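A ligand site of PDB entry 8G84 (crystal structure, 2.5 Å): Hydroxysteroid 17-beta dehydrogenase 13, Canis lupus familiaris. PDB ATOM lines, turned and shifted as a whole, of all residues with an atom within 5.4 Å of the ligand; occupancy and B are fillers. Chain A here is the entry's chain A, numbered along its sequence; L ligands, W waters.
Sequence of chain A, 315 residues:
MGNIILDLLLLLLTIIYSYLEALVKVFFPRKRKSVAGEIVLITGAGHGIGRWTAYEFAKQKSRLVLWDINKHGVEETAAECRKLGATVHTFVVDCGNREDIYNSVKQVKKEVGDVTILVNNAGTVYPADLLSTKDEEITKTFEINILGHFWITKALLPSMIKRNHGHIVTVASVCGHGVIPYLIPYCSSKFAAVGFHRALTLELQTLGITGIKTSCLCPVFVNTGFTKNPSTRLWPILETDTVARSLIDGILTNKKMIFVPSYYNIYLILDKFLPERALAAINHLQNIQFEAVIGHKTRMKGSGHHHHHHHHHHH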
ATOM      1  N   THR A  43      14.813 -22.408  27.736  1.00  0.00           N
ATOM      2  CA  THR A  43      13.661 -22.034  26.899  1.00  0.00           C
ATOM      3  C   THR A  43      14.015 -22.257  25.436  1.00  0.00           C
ATOM      4  O   THR A  43      15.184 -22.133  25.070  1.00  0.00           O
ATOM      5  CB  THR A  43      13.183 -20.611  27.174  1.00  0.00           C
ATOM      6  OG1 THR A  43      14.101 -19.674  26.625  1.00  0.00           O
ATOM      7  CG2 THR A  43      12.968 -20.352  28.665  1.00  0.00           C
ATOM      8  N   GLY A  44      13.028 -22.555  24.605  1.00  0.00           N
ATOM      9  CA  GLY A  44      13.263 -22.863  23.206  1.00  0.00           C
ATOM     10  C   GLY A  44      14.038 -24.167  23.037  1.00  0.00           C
ATOM     11  O   GLY A  44      14.759 -24.345  22.052  1.00  0.00           O
ATOM     12  N   ALA A  45      13.883 -25.112  24.002  1.00  0.00           N
ATOM     13  CA  ALA A  45      14.590 -26.405  24.005  1.00  0.00           C
ATOM     14  C   ALA A  45      14.033 -27.456  23.051  1.00  0.00           C
ATOM     15  O   ALA A  45      14.484 -28.593  23.063  1.00  0.00           O
ATOM     16  CB  ALA A  45      14.626 -26.955  25.415  1.00  0.00           C
ATOM     17  N   GLY A  46      13.049 -27.106  22.242  1.00  0.00           N
ATOM     18  CA  GLY A  46      12.433 -28.036  21.316  1.00  0.00           C
ATOM     19  C   GLY A  46      13.182 -28.222  20.016  1.00  0.00           C
ATOM     20  O   GLY A  46      12.814 -29.089  19.218  1.00  0.00           O
ATOM     21  N   HIS A  47      14.245 -27.435  19.774  1.00  0.00           N
ATOM     22  CA  HIS A  47      15.020 -27.519  18.538  1.00  0.00           C
ATOM     23  C   HIS A  47      16.284 -26.641  18.650  1.00  0.00           C
ATOM     24  O   HIS A  47      16.394 -25.847  19.578  1.00  0.00           O
ATOM     25  CB  HIS A  47      14.129 -27.012  17.377  1.00  0.00           C
ATOM     26  CG  HIS A  47      14.711 -27.245  16.021  1.00  0.00           C
ATOM     27  ND1 HIS A  47      15.275 -26.226  15.280  1.00  0.00           N
ATOM     28  CD2 HIS A  47      14.784 -28.390  15.300  1.00  0.00           C
ATOM     29  CE1 HIS A  47      15.678 -26.774  14.163  1.00  0.00           C
ATOM     30  NE2 HIS A  47      15.414 -28.078  14.124  1.00  0.00           N
ATOM     31  N   GLY A  48      17.206 -26.825  17.713  1.00  0.00           N
ATOM     32  CA  GLY A  48      18.416 -26.029  17.556  1.00  0.00           C
ATOM     33  C   GLY A  48      19.338 -25.920  18.753  1.00  0.00           C
ATOM     34  O   GLY A  48      19.646 -26.923  19.402  1.00  0.00           O
ATOM     35  N   ILE A  49      19.821 -24.700  19.020  1.00  0.00           N
ATOM     36  CA  ILE A  49      20.744 -24.433  20.097  1.00  0.00           C
ATOM     37  C   ILE A  49      20.201 -24.879  21.457  1.00  0.00           C
ATOM     38  O   ILE A  49      20.934 -25.478  22.230  1.00  0.00           O
ATOM     39  CB  ILE A  49      21.196 -22.950  20.095  1.00  0.00           C
ATOM     40  CG1 ILE A  49      21.797 -22.554  18.735  1.00  0.00           C
ATOM     41  CG2 ILE A  49      22.166 -22.650  21.246  1.00  0.00           C
ATOM     42  CD1 ILE A  49      21.973 -21.059  18.573  1.00  0.00           C
ATOM     43  N   GLY A  50      18.920 -24.638  21.721  1.00  0.00           N
ATOM     44  CA  GLY A  50      18.311 -25.033  22.981  1.00  0.00           C
ATOM     45  C   GLY A  50      18.302 -26.531  23.177  1.00  0.00           C
ATOM     46  O   GLY A  50      18.560 -27.018  24.283  1.00  0.00           O
ATOM     47  N   TRP A  67      11.367 -25.792  28.216  1.00  0.00           N
ATOM     48  CA  TRP A  67      10.210 -24.982  27.810  1.00  0.00           C
ATOM     49  C   TRP A  67      10.210 -24.740  26.324  1.00  0.00           C
ATOM     50  O   TRP A  67      11.263 -24.470  25.752  1.00  0.00           O
ATOM     51  CB  TRP A  67      10.217 -23.614  28.534  1.00  0.00           C
ATOM     52  CG  TRP A  67       9.721 -23.621  29.952  1.00  0.00           C
ATOM     53  CD1 TRP A  67       9.542 -24.703  30.773  1.00  0.00           C
ATOM     54  CD2 TRP A  67       9.398 -22.471  30.749  1.00  0.00           C
ATOM     55  NE1 TRP A  67       9.115 -24.295  32.010  1.00  0.00           N
ATOM     56  CE2 TRP A  67       9.018 -22.932  32.014  1.00  0.00           C
ATOM     57  CE3 TRP A  67       9.440 -21.089  30.509  1.00  0.00           C
ATOM     58  CZ2 TRP A  67       8.623 -22.070  33.034  1.00  0.00           C
ATOM     59  CZ3 TRP A  67       9.054 -20.233  31.520  1.00  0.00           C
ATOM     60  CH2 TRP A  67       8.640 -20.734  32.758  1.00  0.00           C
ATOM     61  N   ASP A  68       9.039 -24.776  25.699  1.00  0.00           N
ATOM     62  CA  ASP A  68       8.885 -24.488  24.276  1.00  0.00           C
ATOM     63  C   ASP A  68       7.393 -24.379  23.911  1.00  0.00           C
ATOM     64  O   ASP A  68       6.545 -24.910  24.623  1.00  0.00           O
ATOM     65  CB  ASP A  68       9.571 -25.553  23.393  1.00  0.00           C
ATOM     66  CG  ASP A  68      10.024 -25.032  22.041  1.00  0.00           C
ATOM     67  OD1 ASP A  68       9.171 -24.646  21.232  1.00  0.00           O
ATOM     68  OD2 ASP A  68      11.236 -25.011  21.790  1.00  0.00           O
ATOM     69  N   ILE A  69       7.071 -23.672  22.818  1.00  0.00           N
ATOM     70  CA  ILE A  69       5.692 -23.620  22.306  1.00  0.00           C
ATOM     71  C   ILE A  69       5.381 -24.900  21.466  1.00  0.00           C
ATOM     72  O   ILE A  69       4.210 -25.268  21.302  1.00  0.00           O
ATOM     73  CB  ILE A  69       5.452 -22.365  21.443  1.00  0.00           C
ATOM     74  CG1 ILE A  69       6.584 -22.174  20.404  1.00  0.00           C
ATOM     75  CG2 ILE A  69       5.262 -21.164  22.326  1.00  0.00           C
ATOM     76  CD1 ILE A  69       6.321 -21.149  19.434  1.00  0.00           C
ATOM     77  N   ASN A  70       6.438 -25.556  20.927  1.00  0.00           N
ATOM     78  CA  ASN A  70       6.359 -26.782  20.155  1.00  0.00           C
ATOM     79  C   ASN A  70       6.462 -27.982  21.113  1.00  0.00           C
ATOM     80  O   ASN A  70       7.580 -28.362  21.483  1.00  0.00           O
ATOM     81  CB  ASN A  70       7.495 -26.798  19.155  1.00  0.00           C
ATOM     82  CG  ASN A  70       7.589 -28.046  18.321  1.00  0.00           C
ATOM     83  OD1 ASN A  70       6.734 -28.935  18.361  1.00  0.00           O
ATOM     84  ND2 ASN A  70       8.663 -28.149  17.553  1.00  0.00           N
ATOM     85  N   VAL A  93       5.227 -23.684  27.032  1.00  0.00           N
ATOM     86  CA  VAL A  93       5.130 -22.304  27.497  1.00  0.00           C
ATOM     87  C   VAL A  93       5.434 -21.326  26.403  1.00  0.00           C
ATOM     88  O   VAL A  93       6.435 -21.489  25.723  1.00  0.00           O
ATOM     89  CB  VAL A  93       6.138 -22.057  28.683  1.00  0.00           C
ATOM     90  CG1 VAL A  93       5.961 -20.667  29.280  1.00  0.00           C
ATOM     91  CG2 VAL A  93       6.029 -23.141  29.755  1.00  0.00           C
ATOM     92  N   ASP A  94       4.621 -20.279  26.251  1.00  0.00           N
ATOM     93  CA  ASP A  94       4.906 -19.205  25.321  1.00  0.00           C
ATOM     94  C   ASP A  94       5.824 -18.281  26.091  1.00  0.00           C
ATOM     95  O   ASP A  94       5.391 -17.621  27.038  1.00  0.00           O
ATOM     96  CB  ASP A  94       3.644 -18.471  24.880  1.00  0.00           C
ATOM     97  CG  ASP A  94       3.901 -17.293  23.934  1.00  0.00           C
ATOM     98  OD1 ASP A  94       5.078 -17.068  23.563  1.00  0.00           O
ATOM     99  OD2 ASP A  94       2.928 -16.590  23.583  1.00  0.00           O
ATOM    100  N   CYS A  95       7.102 -18.251  25.705  1.00  0.00           N
ATOM    101  CA  CYS A  95       8.098 -17.460  26.398  1.00  0.00           C
ATOM    102  C   CYS A  95       8.094 -15.969  26.037  1.00  0.00           C
ATOM    103  O   CYS A  95       8.964 -15.225  26.480  1.00  0.00           O
ATOM    104  CB  CYS A  95       9.478 -18.082  26.255  1.00  0.00           C
ATOM    105  SG  CYS A  95       9.622 -19.704  27.065  1.00  0.00           S
ATOM    106  N   GLY A  96       7.070 -15.539  25.310  1.00  0.00           N
ATOM    107  CA  GLY A  96       6.832 -14.140  25.008  1.00  0.00           C
ATOM    108  C   GLY A  96       5.612 -13.626  25.762  1.00  0.00           C
ATOM    109  O   GLY A  96       5.363 -12.423  25.753  1.00  0.00           O
ATOM    110  N   ASN A 121      17.041 -18.958  25.894  1.00  0.00           N
ATOM    111  CA  ASN A 121      17.400 -19.281  24.520  1.00  0.00           C
ATOM    112  C   ASN A 121      16.284 -18.972  23.484  1.00  0.00           C
ATOM    113  O   ASN A 121      16.596 -18.520  22.384  1.00  0.00           O
ATOM    114  CB  ASN A 121      17.866 -20.735  24.454  1.00  0.00           C
ATOM    115  CG  ASN A 121      18.032 -21.237  23.063  1.00  0.00           C
ATOM    116  OD1 ASN A 121      19.069 -21.040  22.438  1.00  0.00           O
ATOM    117  ND2 ASN A 121      17.001 -21.863  22.537  1.00  0.00           N
ATOM    118  N   ALA A 122      14.994 -19.195  23.782  1.00  0.00           N
ATOM    119  CA  ALA A 122      13.890 -18.929  22.846  1.00  0.00           C
ATOM    120  C   ALA A 122      14.068 -17.626  22.044  1.00  0.00           C
ATOM    121  O   ALA A 122      14.493 -16.629  22.610  1.00  0.00           O
ATOM    122  CB  ALA A 122      12.569 -18.889  23.602  1.00  0.00           C
ATOM    123  N   GLY A 123      13.883 -17.706  20.732  1.00  0.00           N
ATOM    124  CA  GLY A 123      14.051 -16.560  19.862  1.00  0.00           C
ATOM    125  C   GLY A 123      13.222 -16.637  18.602  1.00  0.00           C
ATOM    126  O   GLY A 123      12.736 -17.707  18.238  1.00  0.00           O
ATOM    127  N   THR A 124      13.042 -15.512  17.938  1.00  0.00           N
ATOM    128  CA  THR A 124      12.282 -15.431  16.692  1.00  0.00           C
ATOM    129  C   THR A 124      12.860 -14.380  15.756  1.00  0.00           C
ATOM    130  O   THR A 124      13.512 -13.427  16.217  1.00  0.00           O
ATOM    131  CB  THR A 124      10.796 -15.149  16.989  1.00  0.00           C
ATOM    132  OG1 THR A 124       9.996 -15.522  15.859  1.00  0.00           O
ATOM    133  CG2 THR A 124      10.544 -13.702  17.378  1.00  0.00           C
ATOM    134  N   ILE A 144       9.522 -11.934  22.605  1.00  0.00           N
ATOM    135  CA  ILE A 144      10.281 -13.173  22.820  1.00  0.00           C
ATOM    136  C   ILE A 144      11.783 -12.917  23.079  1.00  0.00           C
ATOM    137  O   ILE A 144      12.341 -13.488  24.024  1.00  0.00           O
ATOM    138  CB  ILE A 144      10.111 -14.156  21.634  1.00  0.00           C
ATOM    139  CG1 ILE A 144       8.647 -14.508  21.397  1.00  0.00           C
ATOM    140  CG2 ILE A 144      10.991 -15.416  21.824  1.00  0.00           C
ATOM    141  CD1 ILE A 144       8.429 -15.254  20.175  1.00  0.00           C
ATOM    142  N   ASN A 145      12.434 -12.129  22.217  1.00  0.00           N
ATOM    143  CA  ASN A 145      13.884 -11.941  22.293  1.00  0.00           C
ATOM    144  C   ASN A 145      14.380 -11.148  23.482  1.00  0.00           C
ATOM    145  O   ASN A 145      15.550 -11.294  23.804  1.00  0.00           O
ATOM    146  CB  ASN A 145      14.461 -11.356  21.001  1.00  0.00           C
ATOM    147  CG  ASN A 145      14.258 -12.229  19.778  1.00  0.00           C
ATOM    148  OD1 ASN A 145      13.732 -13.351  19.850  1.00  0.00           O
ATOM    149  ND2 ASN A 145      14.666 -11.751  18.622  1.00  0.00           N
ATOM    150  N   VAL A 171      20.998 -15.916  25.605  1.00  0.00           N
ATOM    151  CA  VAL A 171      21.410 -16.218  24.245  1.00  0.00           C
ATOM    152  C   VAL A 171      21.077 -15.009  23.401  1.00  0.00           C
ATOM    153  O   VAL A 171      19.904 -14.715  23.173  1.00  0.00           O
ATOM    154  CB  VAL A 171      20.833 -17.524  23.676  1.00  0.00           C
ATOM    155  CG1 VAL A 171      21.264 -17.681  22.220  1.00  0.00           C
ATOM    156  CG2 VAL A 171      21.278 -18.706  24.519  1.00  0.00           C
ATOM    157  N   ALA A 172      22.098 -14.247  23.003  1.00  0.00           N
ATOM    158  CA  ALA A 172      21.879 -13.054  22.186  1.00  0.00           C
ATOM    159  C   ALA A 172      22.320 -13.366  20.702  1.00  0.00           C
ATOM    160  O   ALA A 172      21.677 -14.232  20.119  1.00  0.00           O
ATOM    161  CB  ALA A 172      22.517 -11.799  22.843  1.00  0.00           C
ATOM    162  N   SER A 173      23.409 -12.837  20.143  1.00  0.00           N
ATOM    163  CA  SER A 173      23.832 -13.066  18.779  1.00  0.00           C
ATOM    164  C   SER A 173      24.999 -12.090  18.542  1.00  0.00           C
ATOM    165  O   SER A 173      25.207 -11.170  19.352  1.00  0.00           O
ATOM    166  CB  SER A 173      22.687 -12.720  17.838  1.00  0.00           C
ATOM    167  OG  SER A 173      23.084 -12.703  16.483  1.00  0.00           O
ATOM    168  N   VAL A 174      25.745 -12.249  17.432  1.00  0.00           N
ATOM    169  CA  VAL A 174      26.708 -11.216  17.051  1.00  0.00           C
ATOM    170  C   VAL A 174      25.908  -9.938  16.626  1.00  0.00           C
ATOM    171  O   VAL A 174      26.448  -8.844  16.668  1.00  0.00           O
ATOM    172  CB  VAL A 174      27.703 -11.682  15.991  1.00  0.00           C
ATOM    173  CG1 VAL A 174      28.625 -12.749  16.569  1.00  0.00           C
ATOM    174  CG2 VAL A 174      26.980 -12.180  14.747  1.00  0.00           C
ATOM    175  N   TYR A 186      15.417  -7.369  14.700  1.00  0.00           N
ATOM    176  CA  TYR A 186      16.183  -8.461  15.270  1.00  0.00           C
ATOM    177  C   TYR A 186      17.442  -7.931  15.933  1.00  0.00           C
ATOM    178  O   TYR A 186      17.671  -8.208  17.101  1.00  0.00           O
ATOM    179  CB  TYR A 186      16.502  -9.503  14.201  1.00  0.00           C
ATOM    180  CG  TYR A 186      17.216 -10.715  14.758  1.00  0.00           C
ATOM    181  CD1 TYR A 186      16.529 -11.669  15.494  1.00  0.00           C
ATOM    182  CD2 TYR A 186      18.572 -10.884  14.567  1.00  0.00           C
ATOM    183  CE1 TYR A 186      17.185 -12.787  15.992  1.00  0.00           C
ATOM    184  CE2 TYR A 186      19.238 -11.994  15.069  1.00  0.00           C
ATOM    185  CZ  TYR A 186      18.544 -12.949  15.778  1.00  0.00           C
ATOM    186  OH  TYR A 186      19.214 -14.044  16.264  1.00  0.00           O
ATOM    187  N   LYS A 190      18.370  -7.891  19.887  1.00  0.00           N
ATOM    188  CA  LYS A 190      19.564  -8.584  20.324  1.00  0.00           C
ATOM    189  C   LYS A 190      20.530  -7.639  21.051  1.00  0.00           C
ATOM    190  O   LYS A 190      21.234  -8.066  21.983  1.00  0.00           O
ATOM    191  CB  LYS A 190      20.214  -9.366  19.166  1.00  0.00           C
ATOM    192  CG  LYS A 190      19.364 -10.527  18.691  1.00  0.00           C
ATOM    193  CD  LYS A 190      19.221 -11.586  19.801  1.00  0.00           C
ATOM    194  CE  LYS A 190      18.414 -12.779  19.395  1.00  0.00           C
ATOM    195  NZ  LYS A 190      18.596 -13.920  20.323  1.00  0.00           N
ATOM    196  N   PRO A 219      26.604 -16.215  18.963  1.00  0.00           N
ATOM    197  CA  PRO A 219      27.082 -16.896  17.755  1.00  0.00           C
ATOM    198  C   PRO A 219      26.853 -16.084  16.480  1.00  0.00           C
ATOM    199  O   PRO A 219      26.048 -15.159  16.452  1.00  0.00           O
ATOM    200  CB  PRO A 219      26.224 -18.176  17.694  1.00  0.00           C
ATOM    201  CG  PRO A 219      25.254 -18.092  18.830  1.00  0.00           C
ATOM    202  CD  PRO A 219      25.264 -16.687  19.354  1.00  0.00           C
ATOM    203  N   VAL A 220      27.544 -16.471  15.412  1.00  0.00           N
ATOM    204  CA  VAL A 220      27.331 -15.963  14.059  1.00  0.00           C
ATOM    205  C   VAL A 220      26.223 -16.903  13.466  1.00  0.00           C
ATOM    206  O   VAL A 220      25.534 -17.553  14.247  1.00  0.00           O
ATOM    207  CB  VAL A 220      28.676 -15.964  13.259  1.00  0.00           C
ATOM    208  CG1 VAL A 220      29.697 -15.012  13.883  1.00  0.00           C
ATOM    209  CG2 VAL A 220      29.241 -17.378  13.150  1.00  0.00           C
ATOM    210  N   PHE A 221      25.987 -16.974  12.124  1.00  0.00           N
ATOM    211  CA  PHE A 221      24.934 -17.852  11.602  1.00  0.00           C
ATOM    212  C   PHE A 221      25.150 -19.319  12.022  1.00  0.00           C
ATOM    213  O   PHE A 221      26.276 -19.795  12.040  1.00  0.00           O
ATOM    214  CB  PHE A 221      24.717 -17.691  10.089  1.00  0.00           C
ATOM    215  CG  PHE A 221      24.171 -16.334   9.673  1.00  0.00           C
ATOM    216  CD1 PHE A 221      22.828 -16.034   9.814  1.00  0.00           C
ATOM    217  CD2 PHE A 221      25.000 -15.386   9.111  1.00  0.00           C
ATOM    218  CE1 PHE A 221      22.329 -14.800   9.403  1.00  0.00           C
ATOM    219  CE2 PHE A 221      24.505 -14.151   8.714  1.00  0.00           C
ATOM    220  CZ  PHE A 221      23.163 -13.865   8.854  1.00  0.00           C
ATOM    221  N   VAL A 222      24.088 -19.938  12.524  1.00  0.00           N
ATOM    222  CA  VAL A 222      24.087 -21.344  12.943  1.00  0.00           C
ATOM    223  C   VAL A 222      23.099 -22.083  12.034  1.00  0.00           C
ATOM    224  O   VAL A 222      22.017 -21.563  11.702  1.00  0.00           O
ATOM    225  CB  VAL A 222      23.771 -21.537  14.441  1.00  0.00           C
ATOM    226  CG1 VAL A 222      24.029 -22.978  14.871  1.00  0.00           C
ATOM    227  CG2 VAL A 222      24.581 -20.577  15.292  1.00  0.00           C
ATOM    228  N   ASN A 223      23.484 -23.279  11.595  1.00  0.00           N
ATOM    229  CA  ASN A 223      22.717 -24.121  10.687  1.00  0.00           C
ATOM    230  C   ASN A 223      21.544 -24.832  11.389  1.00  0.00           C
ATOM    231  O   ASN A 223      21.589 -26.046  11.601  1.00  0.00           O
ATOM    232  CB  ASN A 223      23.656 -25.109  10.034  1.00  0.00           C
ATOM    233  CG  ASN A 223      23.017 -25.956   8.981  1.00  0.00           C
ATOM    234  OD1 ASN A 223      21.996 -25.577   8.393  1.00  0.00           O
ATOM    235  ND2 ASN A 223      23.601 -27.125   8.744  1.00  0.00           N
ATOM    236  N   THR A 224      20.513 -24.065  11.764  1.00  0.00           N
ATOM    237  CA  THR A 224      19.311 -24.594  12.441  1.00  0.00           C
ATOM    238  C   THR A 224      18.024 -24.379  11.615  1.00  0.00           C
ATOM    239  O   THR A 224      16.981 -24.908  11.963  1.00  0.00           O
ATOM    240  CB  THR A 224      19.072 -23.902  13.804  1.00  0.00           C
ATOM    241  OG1 THR A 224      18.852 -22.516  13.599  1.00  0.00           O
ATOM    242  CG2 THR A 224      20.201 -24.123  14.776  1.00  0.00           C
ATOM    243  N   GLY A 225      18.090 -23.550  10.582  1.00  0.00           N
ATOM    244  CA  GLY A 225      16.909 -23.180   9.826  1.00  0.00           C
ATOM    245  C   GLY A 225      16.250 -21.923  10.360  1.00  0.00           C
ATOM    246  O   GLY A 225      15.240 -21.486   9.798  1.00  0.00           O
ATOM    247  N   PHE A 226      16.810 -21.314  11.440  1.00  0.00           N
ATOM    248  CA  PHE A 226      16.332 -20.065  12.057  1.00  0.00           C
ATOM    249  C   PHE A 226      16.241 -18.976  10.981  1.00  0.00           C
ATOM    250  O   PHE A 226      15.236 -18.272  10.895  1.00  0.00           O
ATOM    251  CB  PHE A 226      17.267 -19.677  13.193  1.00  0.00           C
ATOM    252  CG  PHE A 226      16.783 -18.531  14.049  1.00  0.00           C
ATOM    253  CD1 PHE A 226      15.694 -18.671  14.884  1.00  0.00           C
ATOM    254  CD2 PHE A 226      17.456 -17.321  14.051  1.00  0.00           C
ATOM    255  CE1 PHE A 226      15.253 -17.627  15.664  1.00  0.00           C
ATOM    256  CE2 PHE A 226      17.009 -16.277  14.847  1.00  0.00           C
ATOM    257  CZ  PHE A 226      15.904 -16.426  15.621  1.00  0.00           C
ATOM    258  N   THR A 227      17.264 -18.899  10.105  1.00  0.00           N
ATOM    259  CA  THR A 227      17.289 -18.087   8.878  1.00  0.00           C
ATOM    260  C   THR A 227      17.483 -19.079   7.718  1.00  0.00           C
ATOM    261  O   THR A 227      18.192 -20.080   7.854  1.00  0.00           O
ATOM    262  CB  THR A 227      18.323 -16.958   8.909  1.00  0.00           C
ATOM    263  OG1 THR A 227      19.605 -17.496   9.201  1.00  0.00           O
ATOM    264  CG2 THR A 227      17.961 -15.849   9.886  1.00  0.00           C
HETATM  265  P1  LIG L   1      15.518 -22.811  16.071  1.00  0.00           P
HETATM  266  O1  LIG L   1      16.342 -24.008  15.784  1.00  0.00           O
HETATM  267  O2  LIG L   1      14.496 -22.364  15.094  1.00  0.00           O
HETATM  268  O3  LIG L   1      14.770 -23.095  17.440  1.00  0.00           O
HETATM  269  C1  LIG L   1      14.208 -22.021  18.208  1.00  0.00           C
HETATM  270  C2  LIG L   1      13.283 -22.679  19.193  1.00  0.00           C
HETATM  271  O4  LIG L   1      12.640 -21.657  19.985  1.00  0.00           O
HETATM  272  C3  LIG L   1      12.165 -23.499  18.534  1.00  0.00           C
HETATM  273  O5  LIG L   1      12.074 -24.831  19.035  1.00  0.00           O
HETATM  274  C4  LIG L   1      10.908 -22.664  18.801  1.00  0.00           C
HETATM  275  O6  LIG L   1       9.762 -23.488  18.948  1.00  0.00           O
HETATM  276  C5  LIG L   1      11.275 -22.008  20.108  1.00  0.00           C
HETATM  277  N1  LIG L   1      10.508 -20.811  20.416  1.00  0.00           N
HETATM  278  C6  LIG L   1      10.158 -19.825  19.530  1.00  0.00           C
HETATM  279  N2  LIG L   1       9.312 -18.952  20.014  1.00  0.00           N
HETATM  280  C7  LIG L   1       9.084 -19.396  21.310  1.00  0.00           C
HETATM  281  C8  LIG L   1       8.202 -18.960  22.311  1.00  0.00           C
HETATM  282  N3  LIG L   1       7.399 -17.898  22.200  1.00  0.00           N
HETATM  283  N4  LIG L   1       8.146 -19.682  23.464  1.00  0.00           N
HETATM  284  C9  LIG L   1       8.931 -20.767  23.574  1.00  0.00           C
HETATM  285  N5  LIG L   1       9.791 -21.272  22.690  1.00  0.00           N
HETATM  286  C10 LIG L   1       9.821 -20.531  21.566  1.00  0.00           C
HETATM  287  O7  LIG L   1      16.492 -21.592  16.453  1.00  0.00           O
HETATM  288  P2  LIG L   1      17.999 -21.473  16.970  1.00  0.00           P
HETATM  289  O8  LIG L   1      18.314 -22.563  17.912  1.00  0.00           O
HETATM  290  O9  LIG L   1      18.892 -21.238  15.804  1.00  0.00           O
HETATM  291  O10 LIG L   1      17.895 -20.148  17.842  1.00  0.00           O
HETATM  292  C11 LIG L   1      18.005 -20.185  19.286  1.00  0.00           C
HETATM  293  C12 LIG L   1      18.488 -18.846  19.792  1.00  0.00           C
HETATM  294  O11 LIG L   1      19.778 -18.535  19.228  1.00  0.00           O
HETATM  295  C13 LIG L   1      17.587 -17.644  19.463  1.00  0.00           C
HETATM  296  O12 LIG L   1      17.509 -16.731  20.556  1.00  0.00           O
HETATM  297  C14 LIG L   1      18.297 -17.009  18.258  1.00  0.00           C
HETATM  298  O13 LIG L   1      17.906 -15.658  18.100  1.00  0.00           O
HETATM  299  C15 LIG L   1      19.753 -17.251  18.664  1.00  0.00           C
HETATM  300  N6  LIG L   1      20.716 -17.200  17.521  1.00  0.00           N
HETATM  301  C16 LIG L   1      20.518 -17.996  16.463  1.00  0.00           C
HETATM  302  C17 LIG L   1      21.367 -17.923  15.371  1.00  0.00           C
HETATM  303  C18 LIG L   1      21.100 -18.774  14.151  1.00  0.00           C
HETATM  304  O14 LIG L   1      21.630 -18.454  13.068  1.00  0.00           O
HETATM  305  N7  LIG L   1      20.334 -19.839  14.288  1.00  0.00           N
HETATM  306  C19 LIG L   1      22.433 -17.032  15.413  1.00  0.00           C
HETATM  307  C20 LIG L   1      22.614 -16.231  16.526  1.00  0.00           C
HETATM  308  C21 LIG L   1      21.750 -16.341  17.586  1.00  0.00           C
HETATM  309  O   HOH W   1      16.855 -23.146  20.324  1.00  0.00           O
HETATM  310  O   HOH W   2       7.625 -17.916  17.974  1.00  0.00           O
HETATM  311  O   HOH W   3      20.426 -19.396  10.836  1.00  0.00           O
HETATM  312  O   HOH W   4      11.369 -19.219  16.305  1.00  0.00           O
HETATM  313  O   HOH W   5      16.933 -15.447  23.633  1.00  0.00           O
HETATM  314  O   HOH W   6      12.799 -20.617  14.493  1.00  0.00           O
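The backbone NH (N) of His 47 sits close to an oxygen (O5) of the ligand.
A ring nitrogen (ND1) of His 47 lies within hydrogen-bond range of an oxygen (O1) of the ligand, 2.5 Å away.
An oxygen (O9) of the ligand sits at hydrogen-bond distance from the side-chain hydroxyl (OG1) of Thr 224 (2.5 Å).
OD1 of Asp 68 lies within hydrogen-bond range of O6 of the ligand (2.6 Å).
O of Asn 121 lies within hydrogen-bond range of O12 of the ligand.
The side-chain hydroxyl (OH) of Tyr 186 lies within hydrogen-bond range of an oxygen (O13) of the ligand, 2.8 Å away.
The side-chain carboxylate (OD1) of Asp 94 lies within hydrogen-bond range of a nitrogen (N3) of the ligand, 2.8 Å away.
An oxygen (O8) of the ligand is in hydrogen-bond range of the backbone NH (N) of Ile 49, 2.8 Å away.
N4 of the ligand lies within hydrogen-bond range of N of Cys 95 (2.9 Å).
The side-chain amino group of Lys 190 lies within hydrogen-bond range of an oxygen (O13) of the ligand.
The backbone NH (N) of Val 222 lies within hydrogen-bond range of an oxygen (O14) of the ligand (2.9 Å).
The backbone carbonyl oxygen (O) of Asp 68 sits at hydrogen-bond distance from the backbone NH (N) of Val 93, at 3.0 Å.
OD2 of Asp 68 sits at hydrogen-bond distance from N of Gly 46, 2.8 Å away.
N of Gly 50 sits close to ND2 of Asn 121, at 3.5 Å.
The backbone NH of Asn 121 is in hydrogen-bond range of the side-chain hydroxyl of Thr 43.
OD1 of Asp 94 is in hydrogen-bond range of N of Gly 96, 3.1 Å away.
The backbone NH (N) of Gly 44 sits at hydrogen-bond distance from the backbone carbonyl oxygen (O) of Trp 67 (2.8 Å).
The backbone carbonyl oxygen (O) of Pro 219 lies within hydrogen-bond range of the backbone NH (N) of Val 174.
The backbone NH (N) of Ala 122 is in hydrogen-bond range of the side-chain hydroxyl (OG1) of Thr 43 (3.0 Å).
The backbone carbonyl oxygen of Val 93 sits close to a nitrogen (N4) of the ligand (3.4 Å).
Gly 44 touches the ligand.
C of Gly 46 touches O5 of the ligand, at 3.7 Å.
Gly 48 touches the ligand (CA to O1, 3.4 Å).
Ile 69 touches the ligand.
N of Gly 96 touches N3 of the ligand (3.9 Å).
Ala 122 touches the ligand (O to O12, 3.7 Å).
Gly 123 touches the ligand (CA to O12, 3.5 Å).
Ile 144 touches the ligand.
Val 171 touches the ligand.
O of Ala 172 touches C21 of the ligand, 3.3 Å away.
Ser 173 touches the ligand (OG to C20, 3.6 Å).
Pro 219 touches the ligand (O to C20, 3.6 Å).
Val 220 touches the ligand.
CA of Phe 221 touches O14 of the ligand, at 3.7 Å.
Phe 226 touches the ligand.
Water W3 lies within hydrogen-bond range of the side-chain hydroxyl of Thr 227 (2.6 Å), an oxygen (O14) of the ligand (2.7 Å) and the backbone carbonyl oxygen of Val 222 (2.8 Å).
Water W1 lies within hydrogen-bond range of ND2 of Asn 121 (2.6 Å), O of His 47 (2.8 Å), O8 of the ligand (2.9 Å), N of Gly 50 (2.9 Å) and O of Gly 44 (3.0 Å).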
